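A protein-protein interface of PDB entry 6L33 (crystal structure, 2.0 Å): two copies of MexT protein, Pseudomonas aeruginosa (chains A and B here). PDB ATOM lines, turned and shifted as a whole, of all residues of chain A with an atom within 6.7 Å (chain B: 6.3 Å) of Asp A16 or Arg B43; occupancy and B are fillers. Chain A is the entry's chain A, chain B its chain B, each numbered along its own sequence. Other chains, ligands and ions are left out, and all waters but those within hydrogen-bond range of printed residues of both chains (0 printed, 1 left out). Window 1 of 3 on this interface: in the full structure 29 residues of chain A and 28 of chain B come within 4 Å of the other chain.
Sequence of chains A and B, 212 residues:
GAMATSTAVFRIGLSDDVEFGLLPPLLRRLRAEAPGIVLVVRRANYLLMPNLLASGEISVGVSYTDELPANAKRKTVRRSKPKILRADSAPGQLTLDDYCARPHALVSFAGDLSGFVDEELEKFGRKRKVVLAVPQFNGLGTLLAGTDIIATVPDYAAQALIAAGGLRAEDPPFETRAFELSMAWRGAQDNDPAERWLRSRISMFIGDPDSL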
ATOM      1  N   LEU A  14       0.548 -28.596 -29.674  1.00  0.00           N
ATOM      2  CA  LEU A  14      -0.011 -29.289 -28.523  1.00  0.00           C
ATOM      3  C   LEU A  14      -0.035 -28.360 -27.320  1.00  0.00           C
ATOM      4  O   LEU A  14       0.930 -27.633 -27.066  1.00  0.00           O
ATOM      5  CB  LEU A  14       0.793 -30.552 -28.180  1.00  0.00           C
ATOM      6  CG  LEU A  14       1.000 -31.595 -29.283  1.00  0.00           C
ATOM      7  CD1 LEU A  14       1.932 -32.696 -28.802  1.00  0.00           C
ATOM      8  CD2 LEU A  14      -0.324 -32.181 -29.741  1.00  0.00           C
ATOM      9  N   SER A  15      -1.140 -28.390 -26.581  1.00  0.00           N
ATOM     10  CA  SER A  15      -1.199 -27.701 -25.305  1.00  0.00           C
ATOM     11  C   SER A  15      -0.314 -28.420 -24.286  1.00  0.00           C
ATOM     12  O   SER A  15       0.153 -29.540 -24.510  1.00  0.00           O
ATOM     13  CB  SER A  15      -2.643 -27.612 -24.814  1.00  0.00           C
ATOM     14  OG  SER A  15      -3.215 -28.900 -24.671  1.00  0.00           O
ATOM     15  N   ASP A  16      -0.077 -27.754 -23.154  1.00  0.00           N
ATOM     16  CA  ASP A  16       0.871 -28.286 -22.178  1.00  0.00           C
ATOM     17  C   ASP A  16       0.401 -29.623 -21.620  1.00  0.00           C
ATOM     18  O   ASP A  16       1.204 -30.548 -21.450  1.00  0.00           O
ATOM     19  CB  ASP A  16       1.094 -27.276 -21.050  1.00  0.00           C
ATOM     20  CG  ASP A  16       2.316 -27.606 -20.203  1.00  0.00           C
ATOM     21  OD1 ASP A  16       2.247 -28.562 -19.398  1.00  0.00           O
ATOM     22  OD2 ASP A  16       3.347 -26.912 -20.343  1.00  0.00           O
ATOM     23  N   ASP A  17      -0.901 -29.749 -21.349  1.00  0.00           N
ATOM     24  CA  ASP A  17      -1.442 -30.992 -20.803  1.00  0.00           C
ATOM     25  C   ASP A  17      -1.304 -32.144 -21.788  1.00  0.00           C
ATOM     26  O   ASP A  17      -1.079 -33.292 -21.386  1.00  0.00           O
ATOM     27  CB  ASP A  17      -2.911 -30.799 -20.429  1.00  0.00           C
ATOM     28  CG  ASP A  17      -3.713 -30.166 -21.548  1.00  0.00           C
ATOM     29  OD1 ASP A  17      -3.398 -29.018 -21.927  1.00  0.00           O
ATOM     30  OD2 ASP A  17      -4.653 -30.816 -22.054  1.00  0.00           O
ATOM     31  N   VAL A  18      -1.457 -31.863 -23.083  1.00  0.00           N
ATOM     32  CA  VAL A  18      -1.366 -32.916 -24.089  1.00  0.00           C
ATOM     33  C   VAL A  18       0.086 -33.329 -24.299  1.00  0.00           C
ATOM     34  O   VAL A  18       0.406 -34.522 -24.369  1.00  0.00           O
ATOM     35  CB  VAL A  18      -2.021 -32.453 -25.403  1.00  0.00           C
ATOM     36  CG1 VAL A  18      -1.768 -33.462 -26.512  1.00  0.00           C
ATOM     37  CG2 VAL A  18      -3.512 -32.227 -25.199  1.00  0.00           C
ATOM     38  N   GLU A  19       0.986 -32.349 -24.412  1.00  0.00           N
ATOM     39  CA  GLU A  19       2.408 -32.657 -24.539  1.00  0.00           C
ATOM     40  C   GLU A  19       2.907 -33.443 -23.335  1.00  0.00           C
ATOM     41  O   GLU A  19       3.753 -34.335 -23.469  1.00  0.00           O
ATOM     42  CB  GLU A  19       3.211 -31.365 -24.705  1.00  0.00           C
ATOM     43  CG  GLU A  19       4.706 -31.586 -24.881  1.00  0.00           C
ATOM     44  CD  GLU A  19       5.445 -30.322 -25.282  1.00  0.00           C
ATOM     45  OE1 GLU A  19       6.640 -30.196 -24.936  1.00  0.00           O
ATOM     46  OE2 GLU A  19       4.836 -29.455 -25.943  1.00  0.00           O
ATOM     47  N   PHE A  20       2.378 -33.132 -22.151  1.00  0.00           N
ATOM     48  CA  PHE A  20       2.812 -33.802 -20.930  1.00  0.00           C
ATOM     49  C   PHE A  20       2.336 -35.251 -20.892  1.00  0.00           C
ATOM     50  O   PHE A  20       3.141 -36.176 -20.729  1.00  0.00           O
ATOM     51  CB  PHE A  20       2.299 -33.025 -19.717  1.00  0.00           C
ATOM     52  CG  PHE A  20       2.529 -33.714 -18.402  1.00  0.00           C
ATOM     53  CD1 PHE A  20       3.808 -34.055 -17.995  1.00  0.00           C
ATOM     54  CD2 PHE A  20       1.464 -34.004 -17.565  1.00  0.00           C
ATOM     55  CE1 PHE A  20       4.020 -34.682 -16.781  1.00  0.00           C
ATOM     56  CE2 PHE A  20       1.667 -34.632 -16.350  1.00  0.00           C
ATOM     57  CZ  PHE A  20       2.947 -34.972 -15.958  1.00  0.00           C
ATOM     58  N   GLY A  21       1.033 -35.471 -21.061  1.00  0.00           N
ATOM     59  CA  GLY A  21       0.463 -36.782 -20.815  1.00  0.00           C
ATOM     60  C   GLY A  21       0.234 -37.672 -22.020  1.00  0.00           C
ATOM     61  O   GLY A  21       0.151 -38.896 -21.874  1.00  0.00           O
ATOM     62  N   ARG A  43       4.545 -25.652 -28.847  1.00  0.00           N
ATOM     63  CA  ARG A  43       3.740 -25.457 -27.653  1.00  0.00           C
ATOM     64  C   ARG A  43       2.746 -24.328 -27.893  1.00  0.00           C
ATOM     65  O   ARG A  43       3.134 -23.228 -28.298  1.00  0.00           O
ATOM     66  CB  ARG A  43       4.624 -25.141 -26.447  1.00  0.00           C
ATOM     67  CG  ARG A  43       3.887 -25.161 -25.117  1.00  0.00           C
ATOM     68  CD  ARG A  43       4.855 -25.205 -23.945  1.00  0.00           C
ATOM     69  NE  ARG A  43       4.176 -24.996 -22.668  1.00  0.00           N
ATOM     70  CZ  ARG A  43       3.844 -23.803 -22.188  1.00  0.00           C
ATOM     71  NH1 ARG A  43       4.128 -22.706 -22.877  1.00  0.00           N
ATOM     72  NH2 ARG A  43       3.226 -23.705 -21.017  1.00  0.00           N
ATOM     73  N   ALA A  44       1.467 -24.606 -27.660  1.00  0.00           N
ATOM     74  CA  ALA A  44       0.440 -23.582 -27.838  1.00  0.00           C
ATOM     75  C   ALA A  44      -0.760 -23.941 -26.979  1.00  0.00           C
ATOM     76  O   ALA A  44      -1.329 -25.026 -27.136  1.00  0.00           O
ATOM     77  CB  ALA A  44       0.036 -23.455 -29.305  1.00  0.00           C
ATOM     78  N   ASN A  45      -1.137 -23.043 -26.076  1.00  0.00           N
ATOM     79  CA  ASN A  45      -2.345 -23.232 -25.291  1.00  0.00           C
ATOM     80  C   ASN A  45      -3.572 -23.023 -26.181  1.00  0.00           C
ATOM     81  O   ASN A  45      -3.468 -22.702 -27.369  1.00  0.00           O
ATOM     82  CB  ASN A  45      -2.347 -22.289 -24.090  1.00  0.00           C
ATOM     83  CG  ASN A  45      -2.249 -20.829 -24.494  1.00  0.00           C
ATOM     84  OD1 ASN A  45      -3.009 -20.352 -25.337  1.00  0.00           O
ATOM     85  ND2 ASN A  45      -1.309 -20.111 -23.890  1.00  0.00           N
ATOM     86  N   VAL A 107      -3.550 -23.976 -14.006  1.00  0.00           N
ATOM     87  CA  VAL A 107      -2.450 -24.463 -14.831  1.00  0.00           C
ATOM     88  C   VAL A 107      -2.721 -24.125 -16.291  1.00  0.00           C
ATOM     89  O   VAL A 107      -3.699 -24.608 -16.877  1.00  0.00           O
ATOM     90  CB  VAL A 107      -2.223 -25.972 -14.651  1.00  0.00           C
ATOM     91  CG1 VAL A 107      -0.943 -26.393 -15.354  1.00  0.00           C
ATOM     92  CG2 VAL A 107      -2.153 -26.320 -13.170  1.00  0.00           C
ATOM     93  N   SER A 108      -1.859 -23.284 -16.864  1.00  0.00           N
ATOM     94  CA  SER A 108      -1.752 -23.065 -18.309  1.00  0.00           C
ATOM     95  C   SER A 108      -3.029 -22.462 -18.902  1.00  0.00           C
ATOM     96  O   SER A 108      -3.633 -23.004 -19.828  1.00  0.00           O
ATOM     97  CB  SER A 108      -1.379 -24.368 -19.025  1.00  0.00           C
ATOM     98  OG  SER A 108      -0.961 -24.116 -20.355  1.00  0.00           O
ATOM     99  N   PRO A 135       2.367 -22.397 -15.883  1.00  0.00           N
ATOM    100  CA  PRO A 135       2.161 -22.798 -17.280  1.00  0.00           C
ATOM    101  C   PRO A 135       2.326 -24.281 -17.574  1.00  0.00           C
ATOM    102  O   PRO A 135       2.082 -24.687 -18.715  1.00  0.00           O
ATOM    103  CB  PRO A 135       3.247 -21.993 -18.006  1.00  0.00           C
ATOM    104  CG  PRO A 135       4.373 -21.965 -17.029  1.00  0.00           C
ATOM    105  CD  PRO A 135       3.749 -21.931 -15.652  1.00  0.00           C
ATOM    106  N   GLN A 136       2.726 -25.104 -16.607  1.00  0.00           N
ATOM    107  CA  GLN A 136       3.070 -26.487 -16.894  1.00  0.00           C
ATOM    108  C   GLN A 136       2.473 -27.415 -15.850  1.00  0.00           C
ATOM    109  O   GLN A 136       2.300 -27.045 -14.685  1.00  0.00           O
ATOM    110  CB  GLN A 136       4.593 -26.683 -16.956  1.00  0.00           C
ATOM    111  CG  GLN A 136       5.329 -26.294 -15.683  1.00  0.00           C
ATOM    112  CD  GLN A 136       6.826 -26.173 -15.897  1.00  0.00           C
ATOM    113  OE1 GLN A 136       7.276 -25.535 -16.847  1.00  0.00           O
ATOM    114  NE2 GLN A 136       7.604 -26.790 -15.014  1.00  0.00           N
ATOM    115  N   PHE A 137       2.164 -28.637 -16.284  1.00  0.00           N
ATOM    116  CA  PHE A 137       1.643 -29.659 -15.385  1.00  0.00           C
ATOM    117  C   PHE A 137       2.745 -30.483 -14.737  1.00  0.00           C
ATOM    118  O   PHE A 137       2.584 -30.930 -13.595  1.00  0.00           O
ATOM    119  CB  PHE A 137       0.682 -30.586 -16.136  1.00  0.00           C
ATOM    120  CG  PHE A 137      -0.587 -29.915 -16.574  1.00  0.00           C
ATOM    121  CD1 PHE A 137      -0.625 -29.167 -17.741  1.00  0.00           C
ATOM    122  CD2 PHE A 137      -1.739 -30.022 -15.816  1.00  0.00           C
ATOM    123  CE1 PHE A 137      -1.790 -28.542 -18.145  1.00  0.00           C
ATOM    124  CE2 PHE A 137      -2.909 -29.400 -16.215  1.00  0.00           C
ATOM    125  CZ  PHE A 137      -2.936 -28.661 -17.383  1.00  0.00           C
ATOM    126  N   ASN A 138       3.860 -30.691 -15.437  1.00  0.00           N
ATOM    127  CA  ASN A 138       4.959 -31.469 -14.882  1.00  0.00           C
ATOM    128  C   ASN A 138       5.517 -30.783 -13.642  1.00  0.00           C
ATOM    129  O   ASN A 138       5.803 -29.581 -13.654  1.00  0.00           O
ATOM    130  CB  ASN A 138       6.057 -31.657 -15.931  1.00  0.00           C
ATOM    131  CG  ASN A 138       6.877 -32.916 -15.702  1.00  0.00           C
ATOM    132  OD1 ASN A 138       6.708 -33.610 -14.696  1.00  0.00           O
ATOM    133  ND2 ASN A 138       7.769 -33.217 -16.638  1.00  0.00           N
ATOM    134  N   TYR A 156      -5.883 -37.469 -18.306  1.00  0.00           N
ATOM    135  CA  TYR A 156      -4.615 -38.008 -18.790  1.00  0.00           C
ATOM    136  C   TYR A 156      -3.427 -37.350 -18.098  1.00  0.00           C
ATOM    137  O   TYR A 156      -2.392 -37.997 -17.902  1.00  0.00           O
ATOM    138  CB  TYR A 156      -4.504 -37.857 -20.310  1.00  0.00           C
ATOM    139  CG  TYR A 156      -4.906 -36.503 -20.845  1.00  0.00           C
ATOM    140  CD1 TYR A 156      -3.989 -35.462 -20.921  1.00  0.00           C
ATOM    141  CD2 TYR A 156      -6.203 -36.270 -21.289  1.00  0.00           C
ATOM    142  CE1 TYR A 156      -4.356 -34.223 -21.413  1.00  0.00           C
ATOM    143  CE2 TYR A 156      -6.577 -35.038 -21.780  1.00  0.00           C
ATOM    144  CZ  TYR A 156      -5.652 -34.018 -21.842  1.00  0.00           C
ATOM    145  OH  TYR A 156      -6.027 -32.788 -22.333  1.00  0.00           O
ATOM    146  N   ILE B  12       5.575 -13.151 -13.596  1.00  0.00           N
ATOM    147  CA  ILE B  12       6.977 -13.467 -13.827  1.00  0.00           C
ATOM    148  C   ILE B  12       7.075 -14.515 -14.927  1.00  0.00           C
ATOM    149  O   ILE B  12       6.132 -15.262 -15.196  1.00  0.00           O
ATOM    150  CB  ILE B  12       7.688 -13.966 -12.547  1.00  0.00           C
ATOM    151  CG1 ILE B  12       7.198 -15.364 -12.171  1.00  0.00           C
ATOM    152  CG2 ILE B  12       7.473 -12.999 -11.393  1.00  0.00           C
ATOM    153  CD1 ILE B  12       7.908 -15.955 -10.966  1.00  0.00           C
ATOM    154  N   GLY B  13       8.241 -14.560 -15.565  1.00  0.00           N
ATOM    155  CA  GLY B  13       8.530 -15.535 -16.604  1.00  0.00           C
ATOM    156  C   GLY B  13       9.627 -16.482 -16.146  1.00  0.00           C
ATOM    157  O   GLY B  13      10.633 -16.053 -15.581  1.00  0.00           O
ATOM    158  N   LEU B  14       9.417 -17.772 -16.390  1.00  0.00           N
ATOM    159  CA  LEU B  14      10.365 -18.775 -15.931  1.00  0.00           C
ATOM    160  C   LEU B  14      10.633 -19.787 -17.031  1.00  0.00           C
ATOM    161  O   LEU B  14       9.708 -20.239 -17.712  1.00  0.00           O
ATOM    162  CB  LEU B  14       9.854 -19.506 -14.678  1.00  0.00           C
ATOM    163  CG  LEU B  14       9.748 -18.713 -13.373  1.00  0.00           C
ATOM    164  CD1 LEU B  14       9.249 -19.620 -12.258  1.00  0.00           C
ATOM    165  CD2 LEU B  14      11.080 -18.070 -12.998  1.00  0.00           C
ATOM    166  N   SER B  15      11.907 -20.128 -17.201  1.00  0.00           N
ATOM    167  CA  SER B  15      12.267 -21.274 -18.019  1.00  0.00           C
ATOM    168  C   SER B  15      11.667 -22.536 -17.409  1.00  0.00           C
ATOM    169  O   SER B  15      11.499 -22.642 -16.191  1.00  0.00           O
ATOM    170  CB  SER B  15      13.789 -21.393 -18.123  1.00  0.00           C
ATOM    171  OG  SER B  15      14.165 -22.538 -18.865  1.00  0.00           O
ATOM    172  N   ASP B  16      11.324 -23.498 -18.269  1.00  0.00           N
ATOM    173  CA  ASP B  16      10.562 -24.649 -17.793  1.00  0.00           C
ATOM    174  C   ASP B  16      11.382 -25.524 -16.850  1.00  0.00           C
ATOM    175  O   ASP B  16      10.816 -26.163 -15.957  1.00  0.00           O
ATOM    176  CB  ASP B  16      10.024 -25.459 -18.976  1.00  0.00           C
ATOM    177  CG  ASP B  16      11.079 -26.329 -19.630  1.00  0.00           C
ATOM    178  OD1 ASP B  16      11.897 -25.798 -20.406  1.00  0.00           O
ATOM    179  OD2 ASP B  16      11.074 -27.552 -19.382  1.00  0.00           O
ATOM    180  N   GLU B  19      11.631 -23.654 -13.347  1.00  0.00           N
ATOM    181  CA  GLU B  19      10.376 -23.701 -12.605  1.00  0.00           C
ATOM    182  C   GLU B  19      10.340 -24.850 -11.599  1.00  0.00           C
ATOM    183  O   GLU B  19       9.711 -24.727 -10.543  1.00  0.00           O
ATOM    184  CB  GLU B  19       9.211 -23.810 -13.591  1.00  0.00           C
ATOM    185  CG  GLU B  19       7.857 -24.016 -12.955  1.00  0.00           C
ATOM    186  CD  GLU B  19       6.731 -23.482 -13.816  1.00  0.00           C
ATOM    187  OE1 GLU B  19       5.557 -23.793 -13.525  1.00  0.00           O
ATOM    188  OE2 GLU B  19       7.027 -22.751 -14.784  1.00  0.00           O
ATOM    189  N   VAL B  41       2.785 -17.211 -13.385  1.00  0.00           N
ATOM    190  CA  VAL B  41       4.042 -17.612 -14.008  1.00  0.00           C
ATOM    191  C   VAL B  41       3.775 -17.877 -15.482  1.00  0.00           C
ATOM    192  O   VAL B  41       2.916 -18.698 -15.829  1.00  0.00           O
ATOM    193  CB  VAL B  41       4.647 -18.852 -13.331  1.00  0.00           C
ATOM    194  CG1 VAL B  41       5.988 -19.194 -13.966  1.00  0.00           C
ATOM    195  CG2 VAL B  41       4.800 -18.627 -11.834  1.00  0.00           C
ATOM    196  N   ARG B  42       4.507 -17.183 -16.347  1.00  0.00           N
ATOM    197  CA  ARG B  42       4.460 -17.409 -17.783  1.00  0.00           C
ATOM    198  C   ARG B  42       5.703 -18.172 -18.225  1.00  0.00           C
ATOM    199  O   ARG B  42       6.777 -18.040 -17.631  1.00  0.00           O
ATOM    200  CB  ARG B  42       4.367 -16.083 -18.545  1.00  0.00           C
ATOM    201  CG  ARG B  42       3.262 -15.153 -18.064  1.00  0.00           C
ATOM    202  CD  ARG B  42       1.883 -15.770 -18.258  1.00  0.00           C
ATOM    203  NE  ARG B  42       1.712 -16.301 -19.608  1.00  0.00           N
ATOM    204  CZ  ARG B  42       1.415 -15.562 -20.673  1.00  0.00           C
ATOM    205  NH1 ARG B  42       1.249 -14.252 -20.552  1.00  0.00           N
ATOM    206  NH2 ARG B  42       1.285 -16.134 -21.863  1.00  0.00           N
ATOM    207  N   ARG B  43       5.545 -18.981 -19.271  1.00  0.00           N
ATOM    208  CA  ARG B  43       6.672 -19.715 -19.836  1.00  0.00           C
ATOM    209  C   ARG B  43       7.611 -18.756 -20.559  1.00  0.00           C
ATOM    210  O   ARG B  43       7.165 -17.897 -21.327  1.00  0.00           O
ATOM    211  CB  ARG B  43       6.172 -20.793 -20.796  1.00  0.00           C
ATOM    212  CG  ARG B  43       7.259 -21.437 -21.654  1.00  0.00           C
ATOM    213  CD  ARG B  43       8.221 -22.277 -20.820  1.00  0.00           C
ATOM    214  NE  ARG B  43       7.529 -23.299 -20.038  1.00  0.00           N
ATOM    215  CZ  ARG B  43       7.134 -24.472 -20.521  1.00  0.00           C
ATOM    216  NH1 ARG B  43       7.365 -24.782 -21.790  1.00  0.00           N
ATOM    217  NH2 ARG B  43       6.511 -25.340 -19.735  1.00  0.00           N
ATOM    218  N   ALA B  44       8.914 -18.901 -20.315  1.00  0.00           N
ATOM    219  CA  ALA B  44       9.915 -18.016 -20.889  1.00  0.00           C
ATOM    220  C   ALA B  44      11.052 -18.821 -21.499  1.00  0.00           C
ATOM    221  O   ALA B  44      11.435 -19.873 -20.976  1.00  0.00           O
ATOM    222  CB  ALA B  44      10.477 -17.049 -19.838  1.00  0.00           C
ATOM    223  N   ASN B  45      11.579 -18.319 -22.614  1.00  0.00           N
ATOM    224  CA  ASN B  45      12.785 -18.848 -23.237  1.00  0.00           C
ATOM    225  C   ASN B  45      13.531 -17.671 -23.853  1.00  0.00           C
ATOM    226  O   ASN B  45      13.035 -16.543 -23.870  1.00  0.00           O
ATOM    227  CB  ASN B  45      12.459 -19.932 -24.275  1.00  0.00           C
ATOM    228  CG  ASN B  45      11.556 -19.432 -25.390  1.00  0.00           C
ATOM    229  OD1 ASN B  45      11.985 -18.675 -26.261  1.00  0.00           O
ATOM    230  ND2 ASN B  45      10.301 -19.868 -25.377  1.00  0.00           N
ATOM    231  N   LEU B  48      11.371 -15.747 -26.513  1.00  0.00           N
ATOM    232  CA  LEU B  48      10.206 -15.015 -26.031  1.00  0.00           C
ATOM    233  C   LEU B  48      10.560 -13.945 -25.008  1.00  0.00           C
ATOM    234  O   LEU B  48       9.730 -13.070 -24.735  1.00  0.00           O
ATOM    235  CB  LEU B  48       9.195 -15.977 -25.402  1.00  0.00           C
ATOM    236  CG  LEU B  48       8.402 -16.922 -26.303  1.00  0.00           C
ATOM    237  CD1 LEU B  48       7.381 -17.686 -25.475  1.00  0.00           C
ATOM    238  CD2 LEU B  48       7.722 -16.156 -27.426  1.00  0.00           C
ATOM    239  N   LEU B  52       8.239 -10.815 -23.819  1.00  0.00           N
ATOM    240  CA  LEU B  52       7.519 -10.812 -22.549  1.00  0.00           C
ATOM    241  C   LEU B  52       7.780  -9.533 -21.763  1.00  0.00           C
ATOM    242  O   LEU B  52       6.872  -8.996 -21.118  1.00  0.00           O
ATOM    243  CB  LEU B  52       7.910 -12.036 -21.721  1.00  0.00           C
ATOM    244  CG  LEU B  52       7.484 -13.404 -22.258  1.00  0.00           C
ATOM    245  CD1 LEU B  52       8.136 -14.517 -21.456  1.00  0.00           C
ATOM    246  CD2 LEU B  52       5.970 -13.543 -22.243  1.00  0.00           C
ATOM    247  N   PRO B 135       9.420 -28.166 -27.767  1.00  0.00           N
ATOM    248  CA  PRO B 135       9.470 -26.772 -27.301  1.00  0.00           C
ATOM    249  C   PRO B 135       9.885 -26.580 -25.848  1.00  0.00           C
ATOM    250  O   PRO B 135       9.818 -25.448 -25.359  1.00  0.00           O
ATOM    251  CB  PRO B 135       8.019 -26.315 -27.502  1.00  0.00           C
ATOM    252  CG  PRO B 135       7.213 -27.555 -27.261  1.00  0.00           C
ATOM    253  CD  PRO B 135       8.056 -28.723 -27.709  1.00  0.00           C
ATOM    254  N   GLN B 136      10.312 -27.628 -25.147  1.00  0.00           N
ATOM    255  CA  GLN B 136      10.658 -27.503 -23.738  1.00  0.00           C
ATOM    256  C   GLN B 136      11.661 -28.582 -23.361  1.00  0.00           C
ATOM    257  O   GLN B 136      11.921 -29.517 -24.123  1.00  0.00           O
ATOM    258  CB  GLN B 136       9.420 -27.607 -22.846  1.00  0.00           C
ATOM    259  CG  GLN B 136       8.837 -29.004 -22.789  1.00  0.00           C
ATOM    260  CD  GLN B 136       7.429 -29.021 -22.239  1.00  0.00           C
ATOM    261  OE1 GLN B 136       6.733 -28.007 -22.256  1.00  0.00           O
ATOM    262  NE2 GLN B 136       6.998 -30.177 -21.747  1.00  0.00           N
ATOM    263  N   PHE B 137      12.207 -28.447 -22.154  1.00  0.00           N
ATOM    264  CA  PHE B 137      13.193 -29.382 -21.629  1.00  0.00           C
ATOM    265  C   PHE B 137      12.552 -30.557 -20.899  1.00  0.00           C
ATOM    266  O   PHE B 137      12.919 -31.708 -21.142  1.00  0.00           O
ATOM    267  CB  PHE B 137      14.162 -28.649 -20.696  1.00  0.00           C
ATOM    268  CG  PHE B 137      15.107 -27.732 -21.412  1.00  0.00           C
ATOM    269  CD1 PHE B 137      16.099 -28.246 -22.230  1.00  0.00           C
ATOM    270  CD2 PHE B 137      14.997 -26.358 -21.279  1.00  0.00           C
ATOM    271  CE1 PHE B 137      16.972 -27.406 -22.898  1.00  0.00           C
ATOM    272  CE2 PHE B 137      15.870 -25.512 -21.945  1.00  0.00           C
ATOM    273  CZ  PHE B 137      16.858 -26.039 -22.757  1.00  0.00           C
ATOM    274  N   ASN B 138      11.597 -30.289 -20.009  1.00  0.00           N
ATOM    275  CA  ASN B 138      11.033 -31.355 -19.191  1.00  0.00           C
ATOM    276  C   ASN B 138      10.267 -32.356 -20.050  1.00  0.00           C
ATOM    277  O   ASN B 138       9.664 -32.006 -21.069  1.00  0.00           O
ATOM    278  CB  ASN B 138      10.123 -30.783 -18.102  1.00  0.00           C
ATOM    279  CG  ASN B 138       9.025 -29.893 -18.653  1.00  0.00           C
ATOM    280  OD1 ASN B 138       8.120 -30.356 -19.348  1.00  0.00           O
ATOM    281  ND2 ASN B 138       9.088 -28.607 -18.326  1.00  0.00           N
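The side-chain amide nitrogen (NE2) of Gln A136 sits at hydrogen-bond distance from the backbone carbonyl oxygen (O) of Asp B16, 3.4 Å away. The guanidinium group (NH2) of Arg B43 is in hydrogen-bond range of the side-chain amide oxygen (OE1) of Gln A136, 3.0 Å away. NE of Arg A43 lies close to NH1 of Arg B43 (3.3 Å). The side-chain carboxylate (OD2) of Asp A16 is in salt-bridge range of the guanidinium group (NH2) of Arg B43 (3.6 Å). OE1 of Glu A19 lies close to NE2 of Gln B136 (3.2 Å). The side-chain carboxylate (OE2) of Glu B19 lies close to the side-chain amide oxygen (OE1) of Gln A136 (3.5 Å).
The side-chain carboxylate (OD2) of Asp B16 is in hydrogen-bond range of the side-chain amide nitrogen (ND2) of Asn B138 (2.5 Å). The side-chain amide oxygen (OD1) of Asn B138 is in hydrogen-bond range of the side-chain amide nitrogen (NE2) of Gln B136 (2.7 Å). The backbone NH (N) of Phe B137 sits at hydrogen-bond distance from the side-chain carboxylate (OD2) of Asp B16 (3.1 Å). The side-chain carboxylate (OD2) of Asp A16 lies within salt-bridge range of the guanidinium group (NE) of Arg A43. The guanidinium group of Arg B43 lies within hydrogen-bond range of the side-chain amide oxygen of Gln B136 (3.3 Å). The backbone NH (N) of Phe A137 sits at hydrogen-bond distance from the side-chain carboxylate (OD1) of Asp A16.
Among the printed residues, pairs that only touch across the chains: Glu A19 with Pro B135 (3.3 Å), Arg A43 with Pro B135 (3.6 Å), Arg A43 with Gln B136 (3.8 Å), Pro A135 with Glu B19 (3.4 Å), Pro A135 with Val B41 (3.3 Å), Pro A135 with Arg B43 (3.9 Å), Gln A136 with Asn B138 (3.9 Å) and Asn A138 with Asn B138 (3.7 Å).
Asp A16 touches just one residue of chain B: Arg B43. Asn A45 touches none of the printed residues of chain B. Val A107 touches none of the printed residues of chain B. Of the printed residues of chain A, Asp B16 touches Gln A136 (3.4 Å). Of the printed residues of chain A, Glu B19 touches Pro A135 and Gln A136. Of the printed residues of chain A, Val B41 touches Pro A135. Of chain A, only Asp A16 (3.6 Å), Arg A43 (3.3 Å), Pro A135 (3.9 Å) and Gln A136 (3.0 Å) come within 4 Å of Arg B43. Of the printed residues of chain A, Gln B136 touches Glu A19 and Arg A43.
Printed residues of chain A that touch a printed residue of chain B: Asp A16, Glu A19, Arg A43, Pro A135, Gln A136 and Asn A138. Among the printed residues, 14 pairs touch across the chains. Among the printed residues, Asp or Glu carboxylates within 4 Å of a Lys or Arg side-chain nitrogen of the other chain: Asp A16 with Arg B43 (3.6 Å).
Glu A19 touches Gln B136, and with the chains exchanged Gln A136 touches Glu B19. Arg B43 touches its own counterpart, Arg A43. Arg A43 touches Gln B136, and with the chains exchanged Gln A136 touches Arg B43. Asn A138 touches its own counterpart, Asn B138. Positions printed for both chains: 14, 15, 16, 19, 43, 44, 45, 135, 136, 137 and 138.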
